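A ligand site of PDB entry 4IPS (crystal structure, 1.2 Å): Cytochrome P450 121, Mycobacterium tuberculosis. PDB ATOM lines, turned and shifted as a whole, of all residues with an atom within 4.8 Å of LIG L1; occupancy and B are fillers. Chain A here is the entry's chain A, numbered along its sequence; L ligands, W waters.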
ATOM      1  N   LEU A  54     -23.875  11.080   5.372  1.00  0.00           N
ATOM      2  CA  LEU A  54     -24.004  12.303   4.599  1.00  0.00           C
ATOM      3  C   LEU A  54     -24.653  12.117   3.245  1.00  0.00           C
ATOM      4  O   LEU A  54     -25.251  13.066   2.729  1.00  0.00           O
ATOM      5  CB  LEU A  54     -22.657  12.995   4.432  1.00  0.00           C
ATOM      6  CG  LEU A  54     -22.040  13.514   5.740  1.00  0.00           C
ATOM      7  CD1 LEU A  54     -20.665  14.096   5.455  1.00  0.00           C
ATOM      8  CD2 LEU A  54     -22.924  14.564   6.415  1.00  0.00           C
ATOM      9  N   MET A  61     -30.900  17.282   7.781  1.00  0.00           N
ATOM     10  CA  MET A  61     -30.463  18.491   8.487  1.00  0.00           C
ATOM     11  C   MET A  61     -31.686  19.267   8.923  1.00  0.00           C
ATOM     12  O   MET A  61     -31.742  19.702  10.057  1.00  0.00           O
ATOM     13  CB  MET A  61     -29.533  19.435   7.673  1.00  0.00           C
ATOM     14  CG  MET A  61     -29.377  20.891   8.288  1.00  0.00           C
ATOM     15  SD  MET A  61     -28.848  20.983  10.048  1.00  0.00           S
ATOM     16  CE  MET A  61     -27.214  20.245   9.865  1.00  0.00           C
ATOM     17  N   ASN A  84     -31.933  26.585   5.405  1.00  0.00           N
ATOM     18  CA  ASN A  84     -31.588  27.707   4.546  1.00  0.00           C
ATOM     19  C   ASN A  84     -31.377  27.336   3.083  1.00  0.00           C
ATOM     20  O   ASN A  84     -32.001  27.906   2.182  1.00  0.00           O
ATOM     21  CB  ASN A  84     -30.340  28.385   5.097  1.00  0.00           C
ATOM     22  CG  ASN A  84     -30.024  29.746   4.523  1.00  0.00           C
ATOM     23  OD1 ASN A  84     -30.924  30.541   4.251  1.00  0.00           O
ATOM     24  ND2 ASN A  84     -28.741  30.036   4.353  1.00  0.00           N
ATOM     25  N   MET A  85     -30.503  26.345   2.813  1.00  0.00           N
ATOM     26  CA  MET A  85     -30.259  25.971   1.430  1.00  0.00           C
ATOM     27  C   MET A  85     -31.450  25.413   0.718  1.00  0.00           C
ATOM     28  O   MET A  85     -31.661  25.729  -0.464  1.00  0.00           O
ATOM     29  CB  MET A  85     -29.034  25.072   1.291  1.00  0.00           C
ATOM     30  CG  MET A  85     -27.744  25.874   1.318  1.00  0.00           C
ATOM     31  SD  MET A  85     -27.389  26.989  -0.096  1.00  0.00           S
ATOM     32  CE  MET A  85     -28.416  26.266  -1.334  1.00  0.00           C
ATOM     33  N   ILE A 101     -21.058  33.613  -5.737  1.00  0.00           N
ATOM     34  CA  ILE A 101     -20.003  33.339  -4.770  1.00  0.00           C
ATOM     35  C   ILE A 101     -18.810  32.570  -5.345  1.00  0.00           C
ATOM     36  O   ILE A 101     -17.981  32.054  -4.588  1.00  0.00           O
ATOM     37  CB  ILE A 101     -20.593  32.761  -3.458  1.00  0.00           C
ATOM     38  CG1 ILE A 101     -21.115  31.324  -3.671  1.00  0.00           C
ATOM     39  CG2 ILE A 101     -21.666  33.693  -2.848  1.00  0.00           C
ATOM     40  CD1 ILE A 101     -21.572  30.593  -2.417  1.00  0.00           C
ATOM     41  N   HIS A 145     -15.785  38.804   1.834  1.00  0.00           N
ATOM     42  CA  HIS A 145     -17.217  38.649   1.839  1.00  0.00           C
ATOM     43  C   HIS A 145     -17.972  39.941   1.620  1.00  0.00           C
ATOM     44  O   HIS A 145     -19.039  39.915   1.000  1.00  0.00           O
ATOM     45  CB  HIS A 145     -17.694  37.829   3.039  1.00  0.00           C
ATOM     46  CG  HIS A 145     -17.315  36.389   2.899  1.00  0.00           C
ATOM     47  ND1 HIS A 145     -16.045  35.950   3.167  1.00  0.00           N
ATOM     48  CD2 HIS A 145     -18.056  35.349   2.448  1.00  0.00           C
ATOM     49  CE1 HIS A 145     -16.031  34.653   2.855  1.00  0.00           C
ATOM     50  NE2 HIS A 145     -17.223  34.244   2.436  1.00  0.00           N
ATOM     51  N   PHE A 229     -24.935  33.935   4.352  1.00  0.00           N
ATOM     52  CA  PHE A 229     -23.746  33.718   3.532  1.00  0.00           C
ATOM     53  C   PHE A 229     -22.585  34.550   4.037  1.00  0.00           C
ATOM     54  O   PHE A 229     -21.443  34.055   4.044  1.00  0.00           O
ATOM     55  CB  PHE A 229     -24.037  33.927   2.032  1.00  0.00           C
ATOM     56  CG  PHE A 229     -24.607  32.675   1.425  1.00  0.00           C
ATOM     57  CD1 PHE A 229     -25.855  32.189   1.831  1.00  0.00           C
ATOM     58  CD2 PHE A 229     -23.858  31.908   0.551  1.00  0.00           C
ATOM     59  CE1 PHE A 229     -26.338  30.981   1.320  1.00  0.00           C
ATOM     60  CE2 PHE A 229     -24.347  30.686   0.068  1.00  0.00           C
ATOM     61  CZ  PHE A 229     -25.584  30.233   0.459  1.00  0.00           C
ATOM     62  N   ALA A 232     -21.601  32.480   7.489  1.00  0.00           N
ATOM     63  CA  ALA A 232     -21.012  31.162   7.245  1.00  0.00           C
ATOM     64  C   ALA A 232     -19.698  31.308   6.490  1.00  0.00           C
ATOM     65  O   ALA A 232     -18.706  30.650   6.838  1.00  0.00           O
ATOM     66  CB  ALA A 232     -21.987  30.281   6.458  1.00  0.00           C
ATOM     67  N   GLY A 233     -19.662  32.175   5.472  1.00  0.00           N
ATOM     68  CA  GLY A 233     -18.432  32.311   4.727  1.00  0.00           C
ATOM     69  C   GLY A 233     -17.312  32.914   5.540  1.00  0.00           C
ATOM     70  O   GLY A 233     -16.171  32.432   5.497  1.00  0.00           O
ATOM     71  N   SER A 236     -16.117  30.582   8.344  1.00  0.00           N
ATOM     72  CA  SER A 236     -15.483  29.347   7.881  1.00  0.00           C
ATOM     73  C   SER A 236     -14.140  29.608   7.258  1.00  0.00           C
ATOM     74  O   SER A 236     -13.171  28.872   7.520  1.00  0.00           O
ATOM     75  CB  SER A 236     -16.377  28.610   6.911  1.00  0.00           C
ATOM     76  OG  SER A 236     -17.615  28.261   7.519  1.00  0.00           O
ATOM     77  N   THR A 237     -14.039  30.650   6.417  1.00  0.00           N
ATOM     78  CA  THR A 237     -12.771  30.985   5.773  1.00  0.00           C
ATOM     79  C   THR A 237     -11.781  31.571   6.750  1.00  0.00           C
ATOM     80  O   THR A 237     -10.598  31.216   6.698  1.00  0.00           O
ATOM     81  CB  THR A 237     -12.972  31.909   4.562  1.00  0.00           C
ATOM     82  OG1 THR A 237     -13.572  33.143   4.970  1.00  0.00           O
ATOM     83  CG2 THR A 237     -13.778  31.243   3.453  1.00  0.00           C
ATOM     84  N   PHE A 240     -10.716  28.546   9.042  1.00  0.00           N
ATOM     85  CA  PHE A 240      -9.896  27.582   8.340  1.00  0.00           C
ATOM     86  C   PHE A 240      -8.527  28.175   8.034  1.00  0.00           C
ATOM     87  O   PHE A 240      -7.500  27.528   8.278  1.00  0.00           O
ATOM     88  CB  PHE A 240     -10.571  27.096   7.043  1.00  0.00           C
ATOM     89  CG  PHE A 240      -9.595  26.268   6.236  1.00  0.00           C
ATOM     90  CD1 PHE A 240      -9.077  25.088   6.752  1.00  0.00           C
ATOM     91  CD2 PHE A 240      -9.084  26.749   5.031  1.00  0.00           C
ATOM     92  CE1 PHE A 240      -8.071  24.386   6.068  1.00  0.00           C
ATOM     93  CE2 PHE A 240      -8.111  26.025   4.326  1.00  0.00           C
ATOM     94  CZ  PHE A 240      -7.593  24.863   4.875  1.00  0.00           C
ATOM     95  N   LEU A 273      -6.857  21.345   4.175  1.00  0.00           N
ATOM     96  CA  LEU A 273      -8.291  21.108   4.347  1.00  0.00           C
ATOM     97  C   LEU A 273      -8.524  19.715   4.937  1.00  0.00           C
ATOM     98  O   LEU A 273      -9.285  19.557   5.891  1.00  0.00           O
ATOM     99  CB  LEU A 273      -9.037  21.242   3.014  1.00  0.00           C
ATOM    100  CG  LEU A 273      -9.286  22.680   2.565  1.00  0.00           C
ATOM    101  CD1 LEU A 273      -9.572  22.748   1.062  1.00  0.00           C
ATOM    102  CD2 LEU A 273     -10.422  23.327   3.379  1.00  0.00           C
ATOM    103  N   PHE A 279     -13.908  22.446  12.324  1.00  0.00           N
ATOM    104  CA  PHE A 279     -15.259  22.164  12.820  1.00  0.00           C
ATOM    105  C   PHE A 279     -15.170  21.547  14.201  1.00  0.00           C
ATOM    106  O   PHE A 279     -14.573  20.481  14.386  1.00  0.00           O
ATOM    107  CB  PHE A 279     -16.034  21.279  11.841  1.00  0.00           C
ATOM    108  CG  PHE A 279     -16.740  22.055  10.767  1.00  0.00           C
ATOM    109  CD1 PHE A 279     -16.014  22.802   9.854  1.00  0.00           C
ATOM    110  CD2 PHE A 279     -18.122  22.094  10.700  1.00  0.00           C
ATOM    111  CE1 PHE A 279     -16.662  23.566   8.885  1.00  0.00           C
ATOM    112  CE2 PHE A 279     -18.770  22.840   9.698  1.00  0.00           C
ATOM    113  CZ  PHE A 279     -18.040  23.575   8.816  1.00  0.00           C
ATOM    114  N   LEU A 283     -21.098  17.044  12.271  1.00  0.00           N
ATOM    115  CA  LEU A 283     -22.226  17.615  11.533  1.00  0.00           C
ATOM    116  C   LEU A 283     -23.483  16.892  11.985  1.00  0.00           C
ATOM    117  O   LEU A 283     -23.538  15.648  11.940  1.00  0.00           O
ATOM    118  CB  LEU A 283     -22.052  17.414  10.026  1.00  0.00           C
ATOM    119  CG  LEU A 283     -20.764  17.969   9.430  1.00  0.00           C
ATOM    120  CD1 LEU A 283     -20.753  17.739   7.925  1.00  0.00           C
ATOM    121  CD2 LEU A 283     -20.584  19.459   9.755  1.00  0.00           C
ATOM    122  N   ARG A 285     -27.391  15.436  12.115  1.00  0.00           N
ATOM    123  CA  ARG A 285     -28.500  14.987  11.278  1.00  0.00           C
ATOM    124  C   ARG A 285     -29.495  14.292  12.175  1.00  0.00           C
ATOM    125  O   ARG A 285     -29.102  13.610  13.136  1.00  0.00           O
ATOM    126  CB  ARG A 285     -28.039  13.987  10.232  1.00  0.00           C
ATOM    127  CG  ARG A 285     -27.044  14.501   9.193  1.00  0.00           C
ATOM    128  CD  ARG A 285     -27.655  15.547   8.302  1.00  0.00           C
ATOM    129  NE  ARG A 285     -26.782  15.911   7.188  1.00  0.00           N
ATOM    130  CZ  ARG A 285     -25.925  16.940   7.159  1.00  0.00           C
ATOM    131  NH1 ARG A 285     -25.761  17.707   8.233  1.00  0.00           N
ATOM    132  NH2 ARG A 285     -25.230  17.192   6.056  1.00  0.00           N
ATOM    133  N   LEU A 308     -16.049  14.986  11.216  1.00  0.00           N
ATOM    134  CA  LEU A 308     -15.240  15.168  10.008  1.00  0.00           C
ATOM    135  C   LEU A 308     -13.820  14.685  10.141  1.00  0.00           C
ATOM    136  O   LEU A 308     -13.297  14.068   9.200  1.00  0.00           O
ATOM    137  CB  LEU A 308     -15.293  16.622   9.513  1.00  0.00           C
ATOM    138  CG  LEU A 308     -16.684  17.155   9.153  1.00  0.00           C
ATOM    139  CD1 LEU A 308     -16.595  18.593   8.679  1.00  0.00           C
ATOM    140  CD2 LEU A 308     -17.395  16.251   8.136  1.00  0.00           C
ATOM    141  N   LEU A 335     -13.707  15.168   3.535  1.00  0.00           N
ATOM    142  CA  LEU A 335     -15.013  15.698   3.896  1.00  0.00           C
ATOM    143  C   LEU A 335     -14.958  17.094   4.482  1.00  0.00           C
ATOM    144  O   LEU A 335     -15.918  17.497   5.178  1.00  0.00           O
ATOM    145  CB  LEU A 335     -15.710  14.738   4.866  1.00  0.00           C
ATOM    146  CG  LEU A 335     -15.837  13.275   4.391  1.00  0.00           C
ATOM    147  CD1 LEU A 335     -16.754  12.498   5.298  1.00  0.00           C
ATOM    148  CD2 LEU A 335     -16.309  13.138   2.928  1.00  0.00           C
ATOM    149  N   ALA A 336     -13.896  17.860   4.226  1.00  0.00           N
ATOM    150  CA  ALA A 336     -13.830  19.196   4.829  1.00  0.00           C
ATOM    151  C   ALA A 336     -14.969  20.104   4.431  1.00  0.00           C
ATOM    152  O   ALA A 336     -15.282  21.021   5.194  1.00  0.00           O
ATOM    153  CB  ALA A 336     -12.517  19.874   4.509  1.00  0.00           C
ATOM    154  N   PHE A 337     -15.563  19.902   3.243  1.00  0.00           N
ATOM    155  CA  PHE A 337     -16.710  20.684   2.759  1.00  0.00           C
ATOM    156  C   PHE A 337     -18.002  19.864   2.833  1.00  0.00           C
ATOM    157  O   PHE A 337     -19.011  20.226   2.245  1.00  0.00           O
ATOM    158  CB  PHE A 337     -16.462  21.142   1.325  1.00  0.00           C
ATOM    159  CG  PHE A 337     -15.326  22.120   1.190  1.00  0.00           C
ATOM    160  CD1 PHE A 337     -15.388  23.380   1.798  1.00  0.00           C
ATOM    161  CD2 PHE A 337     -14.224  21.808   0.423  1.00  0.00           C
ATOM    162  CE1 PHE A 337     -14.334  24.289   1.647  1.00  0.00           C
ATOM    163  CE2 PHE A 337     -13.189  22.726   0.259  1.00  0.00           C
ATOM    164  CZ  PHE A 337     -13.257  23.966   0.862  1.00  0.00           C
ATOM    165  N   GLY A 338     -17.971  18.773   3.576  1.00  0.00           N
ATOM    166  CA  GLY A 338     -19.133  17.908   3.644  1.00  0.00           C
ATOM    167  C   GLY A 338     -19.247  16.997   2.423  1.00  0.00           C
ATOM    168  O   GLY A 338     -18.258  16.718   1.726  1.00  0.00           O
ATOM    169  N   GLN A 341     -26.173  16.171  -0.151  1.00  0.00           N
ATOM    170  CA  GLN A 341     -27.141  17.245  -0.338  1.00  0.00           C
ATOM    171  C   GLN A 341     -26.652  18.574   0.186  1.00  0.00           C
ATOM    172  O   GLN A 341     -26.964  19.594  -0.433  1.00  0.00           O
ATOM    173  CB  GLN A 341     -28.468  16.870   0.350  1.00  0.00           C
ATOM    174  CG  GLN A 341     -29.613  17.892   0.189  1.00  0.00           C
ATOM    175  CD  GLN A 341     -30.207  17.967  -1.198  1.00  0.00           C
ATOM    176  OE1 GLN A 341     -30.987  18.889  -1.502  1.00  0.00           O
ATOM    177  NE2 GLN A 341     -29.905  17.016  -2.070  1.00  0.00           N
ATOM    178  N   HIS A 342     -25.933  18.583   1.322  1.00  0.00           N
ATOM    179  CA  HIS A 342     -25.529  19.811   1.982  1.00  0.00           C
ATOM    180  C   HIS A 342     -24.083  20.207   1.736  1.00  0.00           C
ATOM    181  O   HIS A 342     -23.530  21.045   2.452  1.00  0.00           O
ATOM    182  CB  HIS A 342     -25.868  19.744   3.464  1.00  0.00           C
ATOM    183  CG  HIS A 342     -27.346  19.628   3.690  1.00  0.00           C
ATOM    184  ND1 HIS A 342     -28.197  20.717   3.479  1.00  0.00           N
ATOM    185  CD2 HIS A 342     -28.100  18.550   3.995  1.00  0.00           C
ATOM    186  CE1 HIS A 342     -29.432  20.267   3.686  1.00  0.00           C
ATOM    187  NE2 HIS A 342     -29.416  18.973   4.013  1.00  0.00           N
ATOM    188  N   PHE A 343     -23.467  19.649   0.687  1.00  0.00           N
ATOM    189  CA  PHE A 343     -22.085  19.995   0.339  1.00  0.00           C
ATOM    190  C   PHE A 343     -21.925  21.523   0.261  1.00  0.00           C
ATOM    191  O   PHE A 343     -22.775  22.215  -0.308  1.00  0.00           O
ATOM    192  CB  PHE A 343     -21.732  19.358  -1.005  1.00  0.00           C
ATOM    193  CG  PHE A 343     -20.310  19.610  -1.395  1.00  0.00           C
ATOM    194  CD1 PHE A 343     -19.287  18.813  -0.899  1.00  0.00           C
ATOM    195  CD2 PHE A 343     -19.971  20.661  -2.242  1.00  0.00           C
ATOM    196  CE1 PHE A 343     -17.954  19.060  -1.217  1.00  0.00           C
ATOM    197  CE2 PHE A 343     -18.631  20.918  -2.547  1.00  0.00           C
ATOM    198  CZ  PHE A 343     -17.630  20.117  -2.047  1.00  0.00           C
ATOM    199  N   CYS A 344     -20.842  22.028   0.840  1.00  0.00           N
ATOM    200  CA  CYS A 344     -20.604  23.461   0.946  1.00  0.00           C
ATOM    201  C   CYS A 344     -20.773  24.205  -0.369  1.00  0.00           C
ATOM    202  O   CYS A 344     -20.027  23.915  -1.299  1.00  0.00           O
ATOM    203  CB  CYS A 344     -19.216  23.712   1.476  1.00  0.00           C
ATOM    204  SG  CYS A 344     -18.851  25.476   1.655  1.00  0.00           S
ATOM    205  N   PRO A 345     -21.674  25.188  -0.457  1.00  0.00           N
ATOM    206  CA  PRO A 345     -21.810  25.962  -1.710  1.00  0.00           C
ATOM    207  C   PRO A 345     -20.656  26.947  -1.923  1.00  0.00           C
ATOM    208  O   PRO A 345     -20.510  27.471  -3.043  1.00  0.00           O
ATOM    209  CB  PRO A 345     -23.150  26.694  -1.543  1.00  0.00           C
ATOM    210  CG  PRO A 345     -23.245  26.886  -0.061  1.00  0.00           C
ATOM    211  CD  PRO A 345     -22.675  25.615   0.531  1.00  0.00           C
ATOM    212  N   GLY A 346     -19.864  27.215  -0.899  1.00  0.00           N
ATOM    213  CA  GLY A 346     -18.748  28.159  -1.021  1.00  0.00           C
ATOM    214  C   GLY A 346     -17.395  27.485  -1.139  1.00  0.00           C
ATOM    215  O   GLY A 346     -16.371  28.153  -0.939  1.00  0.00           O
ATOM    216  N   LEU A 349     -14.694  29.197  -3.314  1.00  0.00           N
ATOM    217  CA  LEU A 349     -14.285  30.463  -2.732  1.00  0.00           C
ATOM    218  C   LEU A 349     -13.413  30.249  -1.501  1.00  0.00           C
ATOM    219  O   LEU A 349     -12.424  30.964  -1.305  1.00  0.00           O
ATOM    220  CB  LEU A 349     -15.516  31.297  -2.416  1.00  0.00           C
ATOM    221  CG  LEU A 349     -15.258  32.723  -1.914  1.00  0.00           C
ATOM    222  CD1 LEU A 349     -14.618  33.582  -2.990  1.00  0.00           C
ATOM    223  CD2 LEU A 349     -16.534  33.350  -1.454  1.00  0.00           C
ATOM    224  N   GLY A 350     -13.765  29.269  -0.670  1.00  0.00           N
ATOM    225  CA  GLY A 350     -12.972  28.930   0.509  1.00  0.00           C
ATOM    226  C   GLY A 350     -11.580  28.470   0.144  1.00  0.00           C
ATOM    227  O   GLY A 350     -10.583  28.902   0.768  1.00  0.00           O
HETATM  228  C1  LIG L   1     -21.975  24.095   4.426  1.00  0.00           C
HETATM  229  C2  LIG L   1     -17.255  23.810   5.360  1.00  0.00           C
HETATM  230  C3  LIG L   1     -16.637  28.133   3.277  1.00  0.00           C
HETATM  231  C4  LIG L   1     -21.405  28.663   3.047  1.00  0.00           C
HETATM  232  C5  LIG L   1     -20.717  23.609   4.760  1.00  0.00           C
HETATM  233  C6  LIG L   1     -20.467  22.248   5.258  1.00  0.00           C
HETATM  234  C7  LIG L   1     -19.158  22.192   5.595  1.00  0.00           C
HETATM  235  C8  LIG L   1     -18.577  23.476   5.239  1.00  0.00           C
HETATM  236  C9  LIG L   1     -18.409  21.041   6.208  1.00  0.00           C
HETATM  237  C10 LIG L   1     -21.497  21.134   5.352  1.00  0.00           C
HETATM  238  C11 LIG L   1     -22.359  21.196   6.593  1.00  0.00           C
HETATM  239  C12 LIG L   1     -23.275  20.029   6.750  1.00  0.00           C
HETATM  240  O1  LIG L   1     -23.419  19.210   5.871  1.00  0.00           O
HETATM  241  O2  LIG L   1     -23.920  19.942   7.881  1.00  0.00           O
HETATM  242  C13 LIG L   1     -16.669  25.047   4.959  1.00  0.00           C
HETATM  243  C14 LIG L   1     -15.262  25.277   4.987  1.00  0.00           C
HETATM  244  C15 LIG L   1     -15.082  26.496   4.346  1.00  0.00           C
HETATM  245  C16 LIG L   1     -16.393  26.968   3.979  1.00  0.00           C
HETATM  246  C17 LIG L   1     -14.225  24.355   5.556  1.00  0.00           C
HETATM  247  C18 LIG L   1     -13.860  27.242   4.074  1.00  0.00           C
HETATM  248  C19 LIG L   1     -12.640  26.806   4.074  1.00  0.00           C
HETATM  249  C20 LIG L   1     -17.886  28.630   2.946  1.00  0.00           C
HETATM  250  C21 LIG L   1     -18.135  29.855   2.239  1.00  0.00           C
HETATM  251  C22 LIG L   1     -19.492  30.061   2.257  1.00  0.00           C
HETATM  252  C23 LIG L   1     -20.072  28.900   2.862  1.00  0.00           C
HETATM  253  C24 LIG L   1     -17.089  30.773   1.685  1.00  0.00           C
HETATM  254  C25 LIG L   1     -20.278  31.177   1.641  1.00  0.00           C
HETATM  255  C26 LIG L   1     -19.826  32.315   1.148  1.00  0.00           C
HETATM  256  C27 LIG L   1     -21.976  27.513   3.522  1.00  0.00           C
HETATM  257  C28 LIG L   1     -23.404  27.291   3.625  1.00  0.00           C
HETATM  258  C29 LIG L   1     -23.569  25.949   3.905  1.00  0.00           C
HETATM  259  C30 LIG L   1     -22.206  25.427   4.074  1.00  0.00           C
HETATM  260  C31 LIG L   1     -24.471  28.326   3.390  1.00  0.00           C
HETATM  261  C32 LIG L   1     -24.884  25.196   4.135  1.00  0.00           C
HETATM  262  C33 LIG L   1     -25.198  24.301   2.922  1.00  0.00           C
HETATM  263  C34 LIG L   1     -26.447  23.369   2.953  1.00  0.00           C
HETATM  264  O3  LIG L   1     -26.757  22.813   1.928  1.00  0.00           O
HETATM  265  O4  LIG L   1     -27.014  23.321   4.086  1.00  0.00           O
HETATM  266  N1  LIG L   1     -19.556  24.331   4.708  1.00  0.00           N
HETATM  267  N2  LIG L   1     -17.349  26.084   4.361  1.00  0.00           N
HETATM  268  N3  LIG L   1     -19.061  28.007   3.273  1.00  0.00           N
HETATM  269  N4  LIG L   1     -21.283  26.387   3.847  1.00  0.00           N
HETATM  270 FE1  LIG L   1     -19.297  26.120   3.854  1.00  0.00          FE
HETATM  271  O1  LG2 L   2     -26.999  28.097   5.713  1.00  0.00           O
HETATM  272  C1  LG2 L   2     -27.172  27.741   6.834  1.00  0.00           C
HETATM  273  C2  LG2 L   2     -27.103  28.681   8.017  1.00  0.00           C
HETATM  274  C3  LG2 L   2     -25.605  28.968   8.504  1.00  0.00           C
HETATM  275  C4  LG2 L   2     -25.581  30.119   9.491  1.00  0.00           C
HETATM  276  C5  LG2 L   2     -25.785  29.910  10.897  1.00  0.00           C
HETATM  277  C6  LG2 L   2     -25.832  30.907  11.812  1.00  0.00           C
HETATM  278  C7  LG2 L   2     -25.653  32.282  11.372  1.00  0.00           C
HETATM  279  O2  LG2 L   2     -25.731  33.247  12.256  1.00  0.00           O
HETATM  280  C8  LG2 L   2     -25.388  32.547   9.986  1.00  0.00           C
HETATM  281  C9  LG2 L   2     -25.311  31.445   9.037  1.00  0.00           C
HETATM  282  N1  LG2 L   2     -27.941  28.245   9.192  1.00  0.00           N
HETATM  283  C10 LG2 L   2     -27.707  26.835   9.517  1.00  0.00           C
HETATM  284  C11 LG2 L   2     -27.632  25.742   8.311  1.00  0.00           C
HETATM  285  N2  LG2 L   2     -27.424  26.450   6.986  1.00  0.00           N
HETATM  286  C12 LG2 L   2     -26.387  24.742   8.476  1.00  0.00           C
HETATM  287  C13 LG2 L   2     -26.216  24.204   9.874  1.00  0.00           C
HETATM  288  C14 LG2 L   2     -27.103  23.327  10.396  1.00  0.00           C
HETATM  289  C15 LG2 L   2     -26.959  22.769  11.745  1.00  0.00           C
HETATM  290  C16 LG2 L   2     -25.866  23.172  12.491  1.00  0.00           C
HETATM  291  O3  LG2 L   2     -25.819  22.580  13.741  1.00  0.00           O
HETATM  292  C17 LG2 L   2     -24.924  24.071  12.035  1.00  0.00           C
HETATM  293  C18 LG2 L   2     -25.120  24.560  10.719  1.00  0.00           C
HETATM  294  O   HOH W   1     -29.156  24.709   4.918  1.00  0.00           O
HETATM  295  O   HOH W   2     -22.464  17.919   3.662  1.00  0.00           O
HETATM  296  O   HOH W   3     -28.754  21.804   0.068  1.00  0.00           O
HETATM  297  O   HOH W   4     -23.877  21.786   9.757  1.00  0.00           O
HETATM  298  O   HOH W   5     -25.444  22.974  -0.382  1.00  0.00           O
HETATM  299  O   HOH W   6     -19.594  26.977   5.996  1.00  0.00           O
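Water W5 lies within hydrogen-bond range of O3 of LIG L1 (2.7 Å) and O of Phe 343 (2.8 Å).
Water W3 bridges the backbone carbonyl oxygen of Gln 341 (2.9 Å) and an oxygen (O3) of LIG L1 (2.9 Å).
Merely in contact with LIG L1: Met 61, Met 85, His 145, Phe 229, Ala 232, Gly 233, Ser 236, Thr 237, Phe 240, Phe 279, Leu 283, Leu 308, Ala 336, Phe 337, Gly 338, Gln 341, Pro 345 and Gly 346.
Of the 29 residues printed, 21 come within 4 Å of LIG L1.
The nearest printed residue that does not touch LIG L1 is Gly 350 (4.04 Å).
An iron atom (FE1) of LIG L1 is bound by the side-chain sulfur (SG) of Cys 344, at 2.3 Å.
O1 of LIG L1 is in salt-bridge range of NH2 of Arg 285 (2.7 Å).
ND1 of His 342 is in hydrogen-bond range of O4 of LIG L1, at 2.9 Å.
O1 of LG2 L2 sits at hydrogen-bond distance from ND2 of Asn 84.
N of Cys 344 sits at hydrogen-bond distance from O of Phe 337 (2.9 Å).
The side-chain sulfur (SG) of Cys 344 lies close to the backbone NH (N) of Gly 346.
OG of Ser 236 lies within hydrogen-bond range of O of Ala 232, 2.7 Å away.
O of Gly 233 sits at hydrogen-bond distance from OG1 of Thr 237 (2.7 Å).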
